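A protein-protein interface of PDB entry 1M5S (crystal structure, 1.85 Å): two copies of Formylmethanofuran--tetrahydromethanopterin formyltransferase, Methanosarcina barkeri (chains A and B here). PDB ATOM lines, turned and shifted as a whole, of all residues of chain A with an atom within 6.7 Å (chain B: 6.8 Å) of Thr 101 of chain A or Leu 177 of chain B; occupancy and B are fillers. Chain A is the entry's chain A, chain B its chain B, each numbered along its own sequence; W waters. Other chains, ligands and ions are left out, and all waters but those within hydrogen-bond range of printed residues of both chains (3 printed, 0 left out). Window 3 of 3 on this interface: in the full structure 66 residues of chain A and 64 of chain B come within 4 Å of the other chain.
Of the 17 printed residues of chain A, 5 touch a printed residue of chain B.
Hydrophobic or aromatic side chains of chain A that line the printed part of chain B: Trp 32 and Pro 100.
Of the 19 printed residues of chain B, 8 touch a printed residue of chain A.
Printed residues of chain B that touch a printed residue of chain A: Gln 173, Leu 177, Glu 181, Ile 201, Ala 203, Ala 243, Val 244 and Tyr 245.
Hydrophobic or aromatic side chains of chain B within 4 Å of the printed part of chain A: Leu 177, Ile 201, Ala 203, Ala 243 and Tyr 245.
Among the printed residues, 16 pairs touch across the chains.
Among the printed residues, no Asp or Glu carboxylate lies within 4 Å of a Lys or Arg side-chain nitrogen of the other chain.
The side-chain hydroxyl (OG1) of Thr 101 of chain A lies within hydrogen-bond range of the backbone NH (N) of Ala 28 of chain A.
The backbone NH of Trp 32 of chain A sits close to the side-chain hydroxyl of Thr 29 of chain A, 3.3 Å away.
O of Thr 101 of chain A sits at hydrogen-bond distance from NH2 of Arg 69 of chain A (2.8 Å).
The side-chain hydroxyl of Thr 102 of chain A is in hydrogen-bond range of the backbone carbonyl oxygen of Ala 99 of chain A (3.1 Å).
N of Thr 101 of chain A sits at hydrogen-bond distance from OE1 of Glu 146 of chain A, at 2.7 Å.
N of Ile 168 of chain B lies within hydrogen-bond range of O of Tyr 245 of chain B, 2.7 Å away.
Printed residues of chain B within 4 Å of Ala 99 of chain A: Ala 203.
Thr 101 of chain A touches just these residues of chain B: Gln 173, Leu 177 and Tyr 245.
Printed residues of chain B within 4 Å of Glu 146 of chain A: Gln 173 (2.9 Å), Ala 203 (3.2 Å), Ala 243 (3.7 Å), Val 244 (3.4 Å) and Tyr 245 (2.7 Å).
Ala 180 of chain B touches none of the printed residues of chain A.
Of the printed residues of chain A, Ile 201 of chain B touches Trp 32 (3.6 Å) and Pro 100 (3.8 Å).
The nearest residue of chain B that does not touch Thr 101 of chain A is Met 174 of chain B (4.5 Å).
Water W1 bridges the side-chain carboxylate of Glu 181 of chain B and the indole nitrogen of Trp 32 of chain A.
Water W3 bridges the side-chain amide oxygen (OE1) of Gln 173 of chain B (2.6 Å) and the guanidinium group (NH1) of Arg 69 of chain A (3.2 Å).
Water W2 lies within hydrogen-bond range of OE2 of Glu 146 of chain A (3.0 Å), NE2 of Gln 173 of chain B (3.1 Å) and O of Asp 148 of chain A (3.1 Å).
No position is printed for both chains.
Of the 16 pairs that touch across the chains among the printed residues, none has its exchanged pair printed and touching as well.
The side-chain amide nitrogen (NE2) of Gln 173 of chain B sits at hydrogen-bond distance from the backbone carbonyl oxygen (O) of Glu 146 of chain A (2.9 Å).
The backbone carbonyl oxygen of Ala 203 of chain B lies within hydrogen-bond range of the backbone NH of Glu 146 of chain A, at 3.2 Å.
N of Glu 146 of chain A lies within hydrogen-bond range of O of Val 244 of chain B (3.4 Å).
OE1 of Glu 146 of chain A lies within hydrogen-bond range of OH of Tyr 245 of chain B, at 2.7 Å.
Among the printed residues, merely in contact across the chains: Thr 101 of chain A with Leu 177 of chain B (3.5 Å), Ala 99 of chain A with Ala 203 of chain B (3.5 Å), Pro 100 of chain A with Leu 177 of chain B (3.6 Å), Trp 32 of chain A with Leu 177 of chain B (3.6 Å), Trp 32 of chain A with Ile 201 of chain B (3.6 Å), Pro 100 of chain A with Ala 203 of chain B (3.7 Å), Glu 146 of chain A with Ala 243 of chain B (3.7 Å), Trp 32 of chain A with Glu 181 of chain B (3.7 Å), Pro 100 of chain A with Ile 201 of chain B (3.8 Å), Thr 101 of chain A with Tyr 245 of chain B (3.8 Å), Thr 101 of chain A with Gln 173 of chain B (3.9 Å) and Pro 100 of chain A with Tyr 245 of chain B (3.9 Å).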
ATOM      1  N   THR A  26      18.371  17.247  37.021  1.00  0.00           N
ATOM      2  CA  THR A  26      18.117  18.147  35.898  1.00  0.00           C
ATOM      3  C   THR A  26      17.049  17.568  34.986  1.00  0.00           C
ATOM      4  O   THR A  26      16.686  16.391  35.107  1.00  0.00           O
ATOM      5  CB  THR A  26      19.376  18.429  35.057  1.00  0.00           C
ATOM      6  OG1 THR A  26      19.727  17.261  34.313  1.00  0.00           O
ATOM      7  CG2 THR A  26      20.553  18.857  35.949  1.00  0.00           C
ATOM      8  N   ALA A  27      16.470  18.429  34.154  1.00  0.00           N
ATOM      9  CA  ALA A  27      15.398  18.033  33.254  1.00  0.00           C
ATOM     10  C   ALA A  27      15.303  19.045  32.128  1.00  0.00           C
ATOM     11  O   ALA A  27      16.037  20.039  32.119  1.00  0.00           O
ATOM     12  CB  ALA A  27      14.077  17.947  34.008  1.00  0.00           C
ATOM     13  N   ALA A  28      14.428  18.769  31.160  1.00  0.00           N
ATOM     14  CA  ALA A  28      14.316  19.605  29.968  1.00  0.00           C
ATOM     15  C   ALA A  28      13.894  21.025  30.340  1.00  0.00           C
ATOM     16  O   ALA A  28      14.397  21.998  29.762  1.00  0.00           O
ATOM     17  CB  ALA A  28      13.317  18.990  28.980  1.00  0.00           C
ATOM     18  N   THR A  29      12.993  21.128  31.325  1.00  0.00           N
ATOM     19  CA  THR A  29      12.490  22.414  31.823  1.00  0.00           C
ATOM     20  C   THR A  29      12.384  22.390  33.345  1.00  0.00           C
ATOM     21  O   THR A  29      12.323  21.314  33.943  1.00  0.00           O
ATOM     22  CB  THR A  29      11.074  22.727  31.272  1.00  0.00           C
ATOM     23  OG1 THR A  29      10.134  21.804  31.837  1.00  0.00           O
ATOM     24  CG2 THR A  29      11.042  22.619  29.745  1.00  0.00           C
ATOM     25  N   TRP A  32       9.617  20.151  34.679  1.00  0.00           N
ATOM     26  CA  TRP A  32       9.852  18.687  34.666  1.00  0.00           C
ATOM     27  C   TRP A  32      10.869  18.288  35.738  1.00  0.00           C
ATOM     28  O   TRP A  32      10.890  17.142  36.211  1.00  0.00           O
ATOM     29  CB  TRP A  32      10.312  18.235  33.284  1.00  0.00           C
ATOM     30  CG  TRP A  32       9.142  18.231  32.311  1.00  0.00           C
ATOM     31  CD1 TRP A  32       9.014  18.967  31.202  1.00  0.00           C
ATOM     32  CD2 TRP A  32       7.980  17.429  32.448  1.00  0.00           C
ATOM     33  NE1 TRP A  32       7.728  18.669  30.652  1.00  0.00           N
ATOM     34  CE2 TRP A  32       7.130  17.779  31.409  1.00  0.00           C
ATOM     35  CE3 TRP A  32       7.565  16.462  33.373  1.00  0.00           C
ATOM     36  CZ2 TRP A  32       5.845  17.247  31.259  1.00  0.00           C
ATOM     37  CZ3 TRP A  32       6.277  15.912  33.198  1.00  0.00           C
ATOM     38  CH2 TRP A  32       5.456  16.291  32.194  1.00  0.00           C
ATOM     39  N   ALA A  33      11.762  19.209  36.075  1.00  0.00           N
ATOM     40  CA  ALA A  33      12.710  18.971  37.154  1.00  0.00           C
ATOM     41  C   ALA A  33      11.967  18.990  38.500  1.00  0.00           C
ATOM     42  O   ALA A  33      12.231  18.157  39.365  1.00  0.00           O
ATOM     43  CB  ALA A  33      13.815  20.031  37.129  1.00  0.00           C
ATOM     44  N   ASP A  67      25.143  19.775  32.995  1.00  0.00           N
ATOM     45  CA  ASP A  67      24.634  19.671  31.631  1.00  0.00           C
ATOM     46  C   ASP A  67      23.973  20.949  31.118  1.00  0.00           C
ATOM     47  O   ASP A  67      23.373  20.954  30.042  1.00  0.00           O
ATOM     48  CB  ASP A  67      23.652  18.489  31.522  1.00  0.00           C
ATOM     49  CG  ASP A  67      22.427  18.647  32.404  1.00  0.00           C
ATOM     50  OD1 ASP A  67      22.316  19.662  33.126  1.00  0.00           O
ATOM     51  OD2 ASP A  67      21.574  17.733  32.381  1.00  0.00           O
ATOM     52  N   ARG A  69      21.412  22.501  32.126  1.00  0.00           N
ATOM     53  CA  ARG A  69      19.946  22.373  32.066  1.00  0.00           C
ATOM     54  C   ARG A  69      19.330  22.799  33.397  1.00  0.00           C
ATOM     55  O   ARG A  69      20.002  22.800  34.439  1.00  0.00           O
ATOM     56  CB  ARG A  69      19.546  20.916  31.822  1.00  0.00           C
ATOM     57  CG  ARG A  69      19.826  20.437  30.398  1.00  0.00           C
ATOM     58  CD  ARG A  69      18.990  19.216  30.005  1.00  0.00           C
ATOM     59  NE  ARG A  69      19.063  18.123  30.989  1.00  0.00           N
ATOM     60  CZ  ARG A  69      18.264  17.046  30.972  1.00  0.00           C
ATOM     61  NH1 ARG A  69      17.322  16.898  30.030  1.00  0.00           N
ATOM     62  NH2 ARG A  69      18.330  16.048  31.866  1.00  0.00           N
ATOM     63  N   VAL A  96      12.785   9.018  39.570  1.00  0.00           N
ATOM     64  CA  VAL A  96      13.557   9.928  38.736  1.00  0.00           C
ATOM     65  C   VAL A  96      13.978   9.275  37.413  1.00  0.00           C
ATOM     66  O   VAL A  96      13.737   9.822  36.334  1.00  0.00           O
ATOM     67  CB  VAL A  96      14.787  10.449  39.501  1.00  0.00           C
ATOM     68  CG1 VAL A  96      15.577  11.416  38.638  1.00  0.00           C
ATOM     69  CG2 VAL A  96      14.343  11.141  40.785  1.00  0.00           C
ATOM     70  N   ALA A  99      10.941   9.268  35.511  1.00  0.00           N
ATOM     71  CA  ALA A  99      10.359  10.581  35.245  1.00  0.00           C
ATOM     72  C   ALA A  99      10.900  11.178  33.945  1.00  0.00           C
ATOM     73  O   ALA A  99      12.071  11.001  33.610  1.00  0.00           O
ATOM     74  CB  ALA A  99      10.647  11.519  36.412  1.00  0.00           C
ATOM     75  N   PRO A 100      10.047  11.902  33.196  1.00  0.00           N
ATOM     76  CA  PRO A 100      10.422  12.508  31.914  1.00  0.00           C
ATOM     77  C   PRO A 100      11.640  13.435  31.966  1.00  0.00           C
ATOM     78  O   PRO A 100      11.689  14.371  32.760  1.00  0.00           O
ATOM     79  CB  PRO A 100       9.162  13.271  31.506  1.00  0.00           C
ATOM     80  CG  PRO A 100       8.060  12.510  32.137  1.00  0.00           C
ATOM     81  CD  PRO A 100       8.613  12.086  33.476  1.00  0.00           C
ATOM     82  N   THR A 101      12.571  13.192  31.048  1.00  0.00           N
ATOM     83  CA  THR A 101      13.703  14.063  30.720  1.00  0.00           C
ATOM     84  C   THR A 101      14.772  14.256  31.792  1.00  0.00           C
ATOM     85  O   THR A 101      15.698  15.048  31.603  1.00  0.00           O
ATOM     86  CB  THR A 101      13.248  15.472  30.234  1.00  0.00           C
ATOM     87  OG1 THR A 101      12.941  16.311  31.360  1.00  0.00           O
ATOM     88  CG2 THR A 101      12.034  15.362  29.327  1.00  0.00           C
ATOM     89  N   THR A 102      14.690  13.496  32.878  1.00  0.00           N
ATOM     90  CA  THR A 102      15.589  13.710  34.003  1.00  0.00           C
ATOM     91  C   THR A 102      17.004  13.190  33.781  1.00  0.00           C
ATOM     92  O   THR A 102      17.225  12.250  33.017  1.00  0.00           O
ATOM     93  CB  THR A 102      15.039  13.057  35.266  1.00  0.00           C
ATOM     94  OG1 THR A 102      14.711  11.692  34.989  1.00  0.00           O
ATOM     95  CG2 THR A 102      13.800  13.790  35.738  1.00  0.00           C
ATOM     96  N   ALA A 103      17.967  13.876  34.388  1.00  0.00           N
ATOM     97  CA  ALA A 103      19.315  13.341  34.590  1.00  0.00           C
ATOM     98  C   ALA A 103      19.658  13.544  36.061  1.00  0.00           C
ATOM     99  O   ALA A 103      19.100  14.426  36.713  1.00  0.00           O
ATOM    100  CB  ALA A 103      20.321  14.073  33.705  1.00  0.00           C
ATOM    101  N   GLU A 146      12.140   6.994  26.448  1.00  0.00           N
ATOM    102  CA  GLU A 146      12.168   8.413  26.105  1.00  0.00           C
ATOM    103  C   GLU A 146      13.463   8.782  25.399  1.00  0.00           C
ATOM    104  O   GLU A 146      13.548   9.828  24.761  1.00  0.00           O
ATOM    105  CB  GLU A 146      12.039   9.269  27.368  1.00  0.00           C
ATOM    106  CG  GLU A 146      13.322   9.318  28.221  1.00  0.00           C
ATOM    107  CD  GLU A 146      13.298  10.394  29.296  1.00  0.00           C
ATOM    108  OE1 GLU A 146      12.314  11.164  29.345  1.00  0.00           O
ATOM    109  OE2 GLU A 146      14.266  10.471  30.089  1.00  0.00           O
ATOM    110  N   ASP A 148      17.937   8.441  26.471  1.00  0.00           N
ATOM    111  CA  ASP A 148      18.971   7.965  27.393  1.00  0.00           C
ATOM    112  C   ASP A 148      18.832   8.666  28.749  1.00  0.00           C
ATOM    113  O   ASP A 148      18.764   9.898  28.816  1.00  0.00           O
ATOM    114  CB  ASP A 148      20.367   8.247  26.823  1.00  0.00           C
ATOM    115  CG  ASP A 148      20.670   7.446  25.560  1.00  0.00           C
ATOM    116  OD1 ASP A 148      20.367   6.233  25.523  1.00  0.00           O
ATOM    117  OD2 ASP A 148      21.308   8.007  24.639  1.00  0.00           O
ATOM    118  N   PHE A 149      18.722   7.881  29.818  1.00  0.00           N
ATOM    119  CA  PHE A 149      18.769   8.428  31.171  1.00  0.00           C
ATOM    120  C   PHE A 149      20.228   8.517  31.633  1.00  0.00           C
ATOM    121  O   PHE A 149      20.980   7.552  31.526  1.00  0.00           O
ATOM    122  CB  PHE A 149      17.955   7.549  32.125  1.00  0.00           C
ATOM    123  CG  PHE A 149      18.074   7.943  33.576  1.00  0.00           C
ATOM    124  CD1 PHE A 149      17.655   9.197  34.010  1.00  0.00           C
ATOM    125  CD2 PHE A 149      18.593   7.049  34.513  1.00  0.00           C
ATOM    126  CE1 PHE A 149      17.746   9.557  35.352  1.00  0.00           C
ATOM    127  CE2 PHE A 149      18.688   7.398  35.865  1.00  0.00           C
ATOM    128  CZ  PHE A 149      18.263   8.657  36.283  1.00  0.00           C
ATOM    129  N   ILE B 168       2.819   6.287  23.580  1.00  0.00           N
ATOM    130  CA  ILE B 168       2.784   7.411  22.647  1.00  0.00           C
ATOM    131  C   ILE B 168       4.108   7.466  21.907  1.00  0.00           C
ATOM    132  O   ILE B 168       5.153   7.683  22.523  1.00  0.00           O
ATOM    133  CB  ILE B 168       2.595   8.765  23.380  1.00  0.00           C
ATOM    134  CG1 ILE B 168       1.326   8.740  24.234  1.00  0.00           C
ATOM    135  CG2 ILE B 168       2.528   9.904  22.365  1.00  0.00           C
ATOM    136  CD1 ILE B 168       1.160   9.974  25.109  1.00  0.00           C
ATOM    137  N   SER B 172       9.803  13.390  18.046  1.00  0.00           N
ATOM    138  CA  SER B 172      10.834  13.934  18.922  1.00  0.00           C
ATOM    139  C   SER B 172      10.437  13.676  20.363  1.00  0.00           C
ATOM    140  O   SER B 172       9.280  13.374  20.640  1.00  0.00           O
ATOM    141  CB  SER B 172      10.989  15.438  18.692  1.00  0.00           C
ATOM    142  OG  SER B 172       9.809  16.126  19.052  1.00  0.00           O
ATOM    143  N   GLN B 173      11.381  13.827  21.284  1.00  0.00           N
ATOM    144  CA  GLN B 173      11.089  13.622  22.700  1.00  0.00           C
ATOM    145  C   GLN B 173      10.004  14.566  23.188  1.00  0.00           C
ATOM    146  O   GLN B 173       9.085  14.157  23.896  1.00  0.00           O
ATOM    147  CB  GLN B 173      12.342  13.823  23.541  1.00  0.00           C
ATOM    148  CG  GLN B 173      12.163  13.477  25.003  1.00  0.00           C
ATOM    149  CD  GLN B 173      13.457  13.566  25.759  1.00  0.00           C
ATOM    150  OE1 GLN B 173      13.971  14.657  25.994  1.00  0.00           O
ATOM    151  NE2 GLN B 173      14.036  12.419  26.081  1.00  0.00           N
ATOM    152  N   MET B 174      10.084  15.821  22.769  1.00  0.00           N
ATOM    153  CA  MET B 174       9.161  16.823  23.278  1.00  0.00           C
ATOM    154  C   MET B 174       7.779  16.729  22.637  1.00  0.00           C
ATOM    155  O   MET B 174       6.778  17.073  23.260  1.00  0.00           O
ATOM    156  CB  MET B 174       9.755  18.224  23.118  1.00  0.00           C
ATOM    157  CG  MET B 174      11.040  18.449  23.924  1.00  0.00           C
ATOM    158  SD  MET B 174      11.032  17.822  25.644  1.00  0.00           S
ATOM    159  CE  MET B 174       9.449  18.326  26.188  1.00  0.00           C
ATOM    160  N   THR B 175       7.716  16.162  21.440  1.00  0.00           N
ATOM    161  CA  THR B 175       6.430  15.857  20.834  1.00  0.00           C
ATOM    162  C   THR B 175       5.713  14.808  21.687  1.00  0.00           C
ATOM    163  O   THR B 175       4.607  15.050  22.179  1.00  0.00           O
ATOM    164  CB  THR B 175       6.598  15.329  19.393  1.00  0.00           C
ATOM    165  OG1 THR B 175       7.109  16.368  18.554  1.00  0.00           O
ATOM    166  CG2 THR B 175       5.272  14.862  18.843  1.00  0.00           C
ATOM    167  N   ALA B 176       6.407  13.709  21.983  1.00  0.00           N
ATOM    168  CA  ALA B 176       5.793  12.610  22.725  1.00  0.00           C
ATOM    169  C   ALA B 176       5.445  13.018  24.158  1.00  0.00           C
ATOM    170  O   ALA B 176       4.393  12.660  24.671  1.00  0.00           O
ATOM    171  CB  ALA B 176       6.715  11.408  22.730  1.00  0.00           C
ATOM    172  N   LEU B 177       6.322  13.791  24.791  1.00  0.00           N
ATOM    173  CA  LEU B 177       6.101  14.226  26.164  1.00  0.00           C
ATOM    174  C   LEU B 177       4.914  15.179  26.263  1.00  0.00           C
ATOM    175  O   LEU B 177       4.118  15.090  27.191  1.00  0.00           O
ATOM    176  CB  LEU B 177       7.354  14.906  26.705  1.00  0.00           C
ATOM    177  CG  LEU B 177       7.306  15.395  28.156  1.00  0.00           C
ATOM    178  CD1 LEU B 177       6.794  14.283  29.061  1.00  0.00           C
ATOM    179  CD2 LEU B 177       8.692  15.836  28.590  1.00  0.00           C
ATOM    180  N   THR B 178       4.779  16.068  25.282  1.00  0.00           N
ATOM    181  CA  THR B 178       3.672  17.020  25.264  1.00  0.00           C
ATOM    182  C   THR B 178       2.345  16.293  25.074  1.00  0.00           C
ATOM    183  O   THR B 178       1.334  16.649  25.692  1.00  0.00           O
ATOM    184  CB  THR B 178       3.862  18.069  24.148  1.00  0.00           C
ATOM    185  OG1 THR B 178       5.106  18.746  24.357  1.00  0.00           O
ATOM    186  CG2 THR B 178       2.733  19.097  24.159  1.00  0.00           C
ATOM    187  N   ALA B 179       2.366  15.249  24.251  1.00  0.00           N
ATOM    188  CA  ALA B 179       1.196  14.396  24.069  1.00  0.00           C
ATOM    189  C   ALA B 179       0.848  13.729  25.399  1.00  0.00           C
ATOM    190  O   ALA B 179      -0.310  13.715  25.814  1.00  0.00           O
ATOM    191  CB  ALA B 179       1.481  13.342  23.007  1.00  0.00           C
ATOM    192  N   ALA B 180       1.869  13.195  26.066  1.00  0.00           N
ATOM    193  CA  ALA B 180       1.711  12.564  27.371  1.00  0.00           C
ATOM    194  C   ALA B 180       1.199  13.555  28.417  1.00  0.00           C
ATOM    195  O   ALA B 180       0.272  13.253  29.169  1.00  0.00           O
ATOM    196  CB  ALA B 180       3.026  11.963  27.813  1.00  0.00           C
ATOM    197  N   GLU B 181       1.780  14.756  28.425  1.00  0.00           N
ATOM    198  CA  GLU B 181       1.327  15.835  29.299  1.00  0.00           C
ATOM    199  C   GLU B 181      -0.155  16.156  29.095  1.00  0.00           C
ATOM    200  O   GLU B 181      -0.913  16.219  30.060  1.00  0.00           O
ATOM    201  CB  GLU B 181       2.168  17.096  29.063  1.00  0.00           C
ATOM    202  CG  GLU B 181       1.622  18.338  29.759  1.00  0.00           C
ATOM    203  CD  GLU B 181       2.584  19.509  29.730  1.00  0.00           C
ATOM    204  OE1 GLU B 181       3.678  19.379  29.138  1.00  0.00           O
ATOM    205  OE2 GLU B 181       2.238  20.565  30.296  1.00  0.00           O
ATOM    206  N   ALA B 182      -0.566  16.319  27.840  1.00  0.00           N
ATOM    207  CA  ALA B 182      -1.966  16.594  27.511  1.00  0.00           C
ATOM    208  C   ALA B 182      -2.896  15.435  27.895  1.00  0.00           C
ATOM    209  O   ALA B 182      -4.007  15.658  28.393  1.00  0.00           O
ATOM    210  CB  ALA B 182      -2.096  16.911  26.023  1.00  0.00           C
ATOM    211  N   ALA B 183      -2.395  14.209  27.768  1.00  0.00           N
ATOM    212  CA  ALA B 183      -3.131  13.016  28.181  1.00  0.00           C
ATOM    213  C   ALA B 183      -3.337  12.931  29.700  1.00  0.00           C
ATOM    214  O   ALA B 183      -4.443  12.664  30.169  1.00  0.00           O
ATOM    215  CB  ALA B 183      -2.410  11.770  27.683  1.00  0.00           C
ATOM    216  N   ILE B 201       3.535  10.035  34.084  1.00  0.00           N
ATOM    217  CA  ILE B 201       4.174   9.617  32.836  1.00  0.00           C
ATOM    218  C   ILE B 201       5.367   8.681  33.059  1.00  0.00           C
ATOM    219  O   ILE B 201       6.290   8.999  33.808  1.00  0.00           O
ATOM    220  CB  ILE B 201       4.645  10.857  32.001  1.00  0.00           C
ATOM    221  CG1 ILE B 201       3.454  11.765  31.676  1.00  0.00           C
ATOM    222  CG2 ILE B 201       5.294  10.413  30.695  1.00  0.00           C
ATOM    223  CD1 ILE B 201       3.850  13.175  31.221  1.00  0.00           C
ATOM    224  N   ALA B 203       8.694   7.336  31.704  1.00  0.00           N
ATOM    225  CA  ALA B 203       9.784   7.679  30.792  1.00  0.00           C
ATOM    226  C   ALA B 203      10.663   6.472  30.495  1.00  0.00           C
ATOM    227  O   ALA B 203      11.421   6.466  29.522  1.00  0.00           O
ATOM    228  CB  ALA B 203      10.628   8.783  31.384  1.00  0.00           C
ATOM    229  N   ALA B 243      11.136   8.929  20.234  1.00  0.00           N
ATOM    230  CA  ALA B 243      10.805   8.859  21.650  1.00  0.00           C
ATOM    231  C   ALA B 243       9.445   8.218  21.885  1.00  0.00           C
ATOM    232  O   ALA B 243       8.522   8.355  21.080  1.00  0.00           O
ATOM    233  CB  ALA B 243      10.837  10.253  22.275  1.00  0.00           C
ATOM    234  N   VAL B 244       9.363   7.448  22.964  1.00  0.00           N
ATOM    235  CA  VAL B 244       8.102   6.863  23.408  1.00  0.00           C
ATOM    236  C   VAL B 244       7.899   7.216  24.886  1.00  0.00           C
ATOM    237  O   VAL B 244       8.858   7.286  25.658  1.00  0.00           O
ATOM    238  CB  VAL B 244       8.086   5.299  23.232  1.00  0.00           C
ATOM    239  CG1 VAL B 244       6.708   4.750  23.560  1.00  0.00           C
ATOM    240  CG2 VAL B 244       8.463   4.915  21.812  1.00  0.00           C
ATOM    241  N   TYR B 245       6.675   7.613  25.218  1.00  0.00           N
ATOM    242  CA  TYR B 245       6.249   7.699  26.604  1.00  0.00           C
ATOM    243  C   TYR B 245       5.037   6.820  26.793  1.00  0.00           C
ATOM    244  O   TYR B 245       4.281   6.569  25.850  1.00  0.00           O
ATOM    245  CB  TYR B 245       5.906   9.136  26.985  1.00  0.00           C
ATOM    246  CG  TYR B 245       7.124   9.998  27.169  1.00  0.00           C
ATOM    247  CD1 TYR B 245       7.845   9.966  28.359  1.00  0.00           C
ATOM    248  CD2 TYR B 245       7.577  10.819  26.145  1.00  0.00           C
ATOM    249  CE1 TYR B 245       8.976  10.726  28.526  1.00  0.00           C
ATOM    250  CE2 TYR B 245       8.714  11.585  26.304  1.00  0.00           C
ATOM    251  CZ  TYR B 245       9.404  11.533  27.502  1.00  0.00           C
ATOM    252  OH  TYR B 245      10.514  12.312  27.686  1.00  0.00           O
ATOM    253  N   VAL B 271      -1.367  16.443  19.258  1.00  0.00           N
ATOM    254  CA  VAL B 271      -0.041  17.065  19.181  1.00  0.00           C
ATOM    255  C   VAL B 271       0.605  16.720  17.845  1.00  0.00           C
ATOM    256  O   VAL B 271       0.845  15.552  17.549  1.00  0.00           O
ATOM    257  CB  VAL B 271       0.913  16.590  20.332  1.00  0.00           C
ATOM    258  CG1 VAL B 271       2.277  17.272  20.201  1.00  0.00           C
ATOM    259  CG2 VAL B 271       0.311  16.909  21.683  1.00  0.00           C
HETATM  260  O   HOH W   1       6.089  20.222  28.943  1.00  0.00           O
HETATM  261  O   HOH W   2      16.240  11.502  28.007  1.00  0.00           O
HETATM  262  O   HOH W   3      15.421  16.106  27.628  1.00  0.00           O
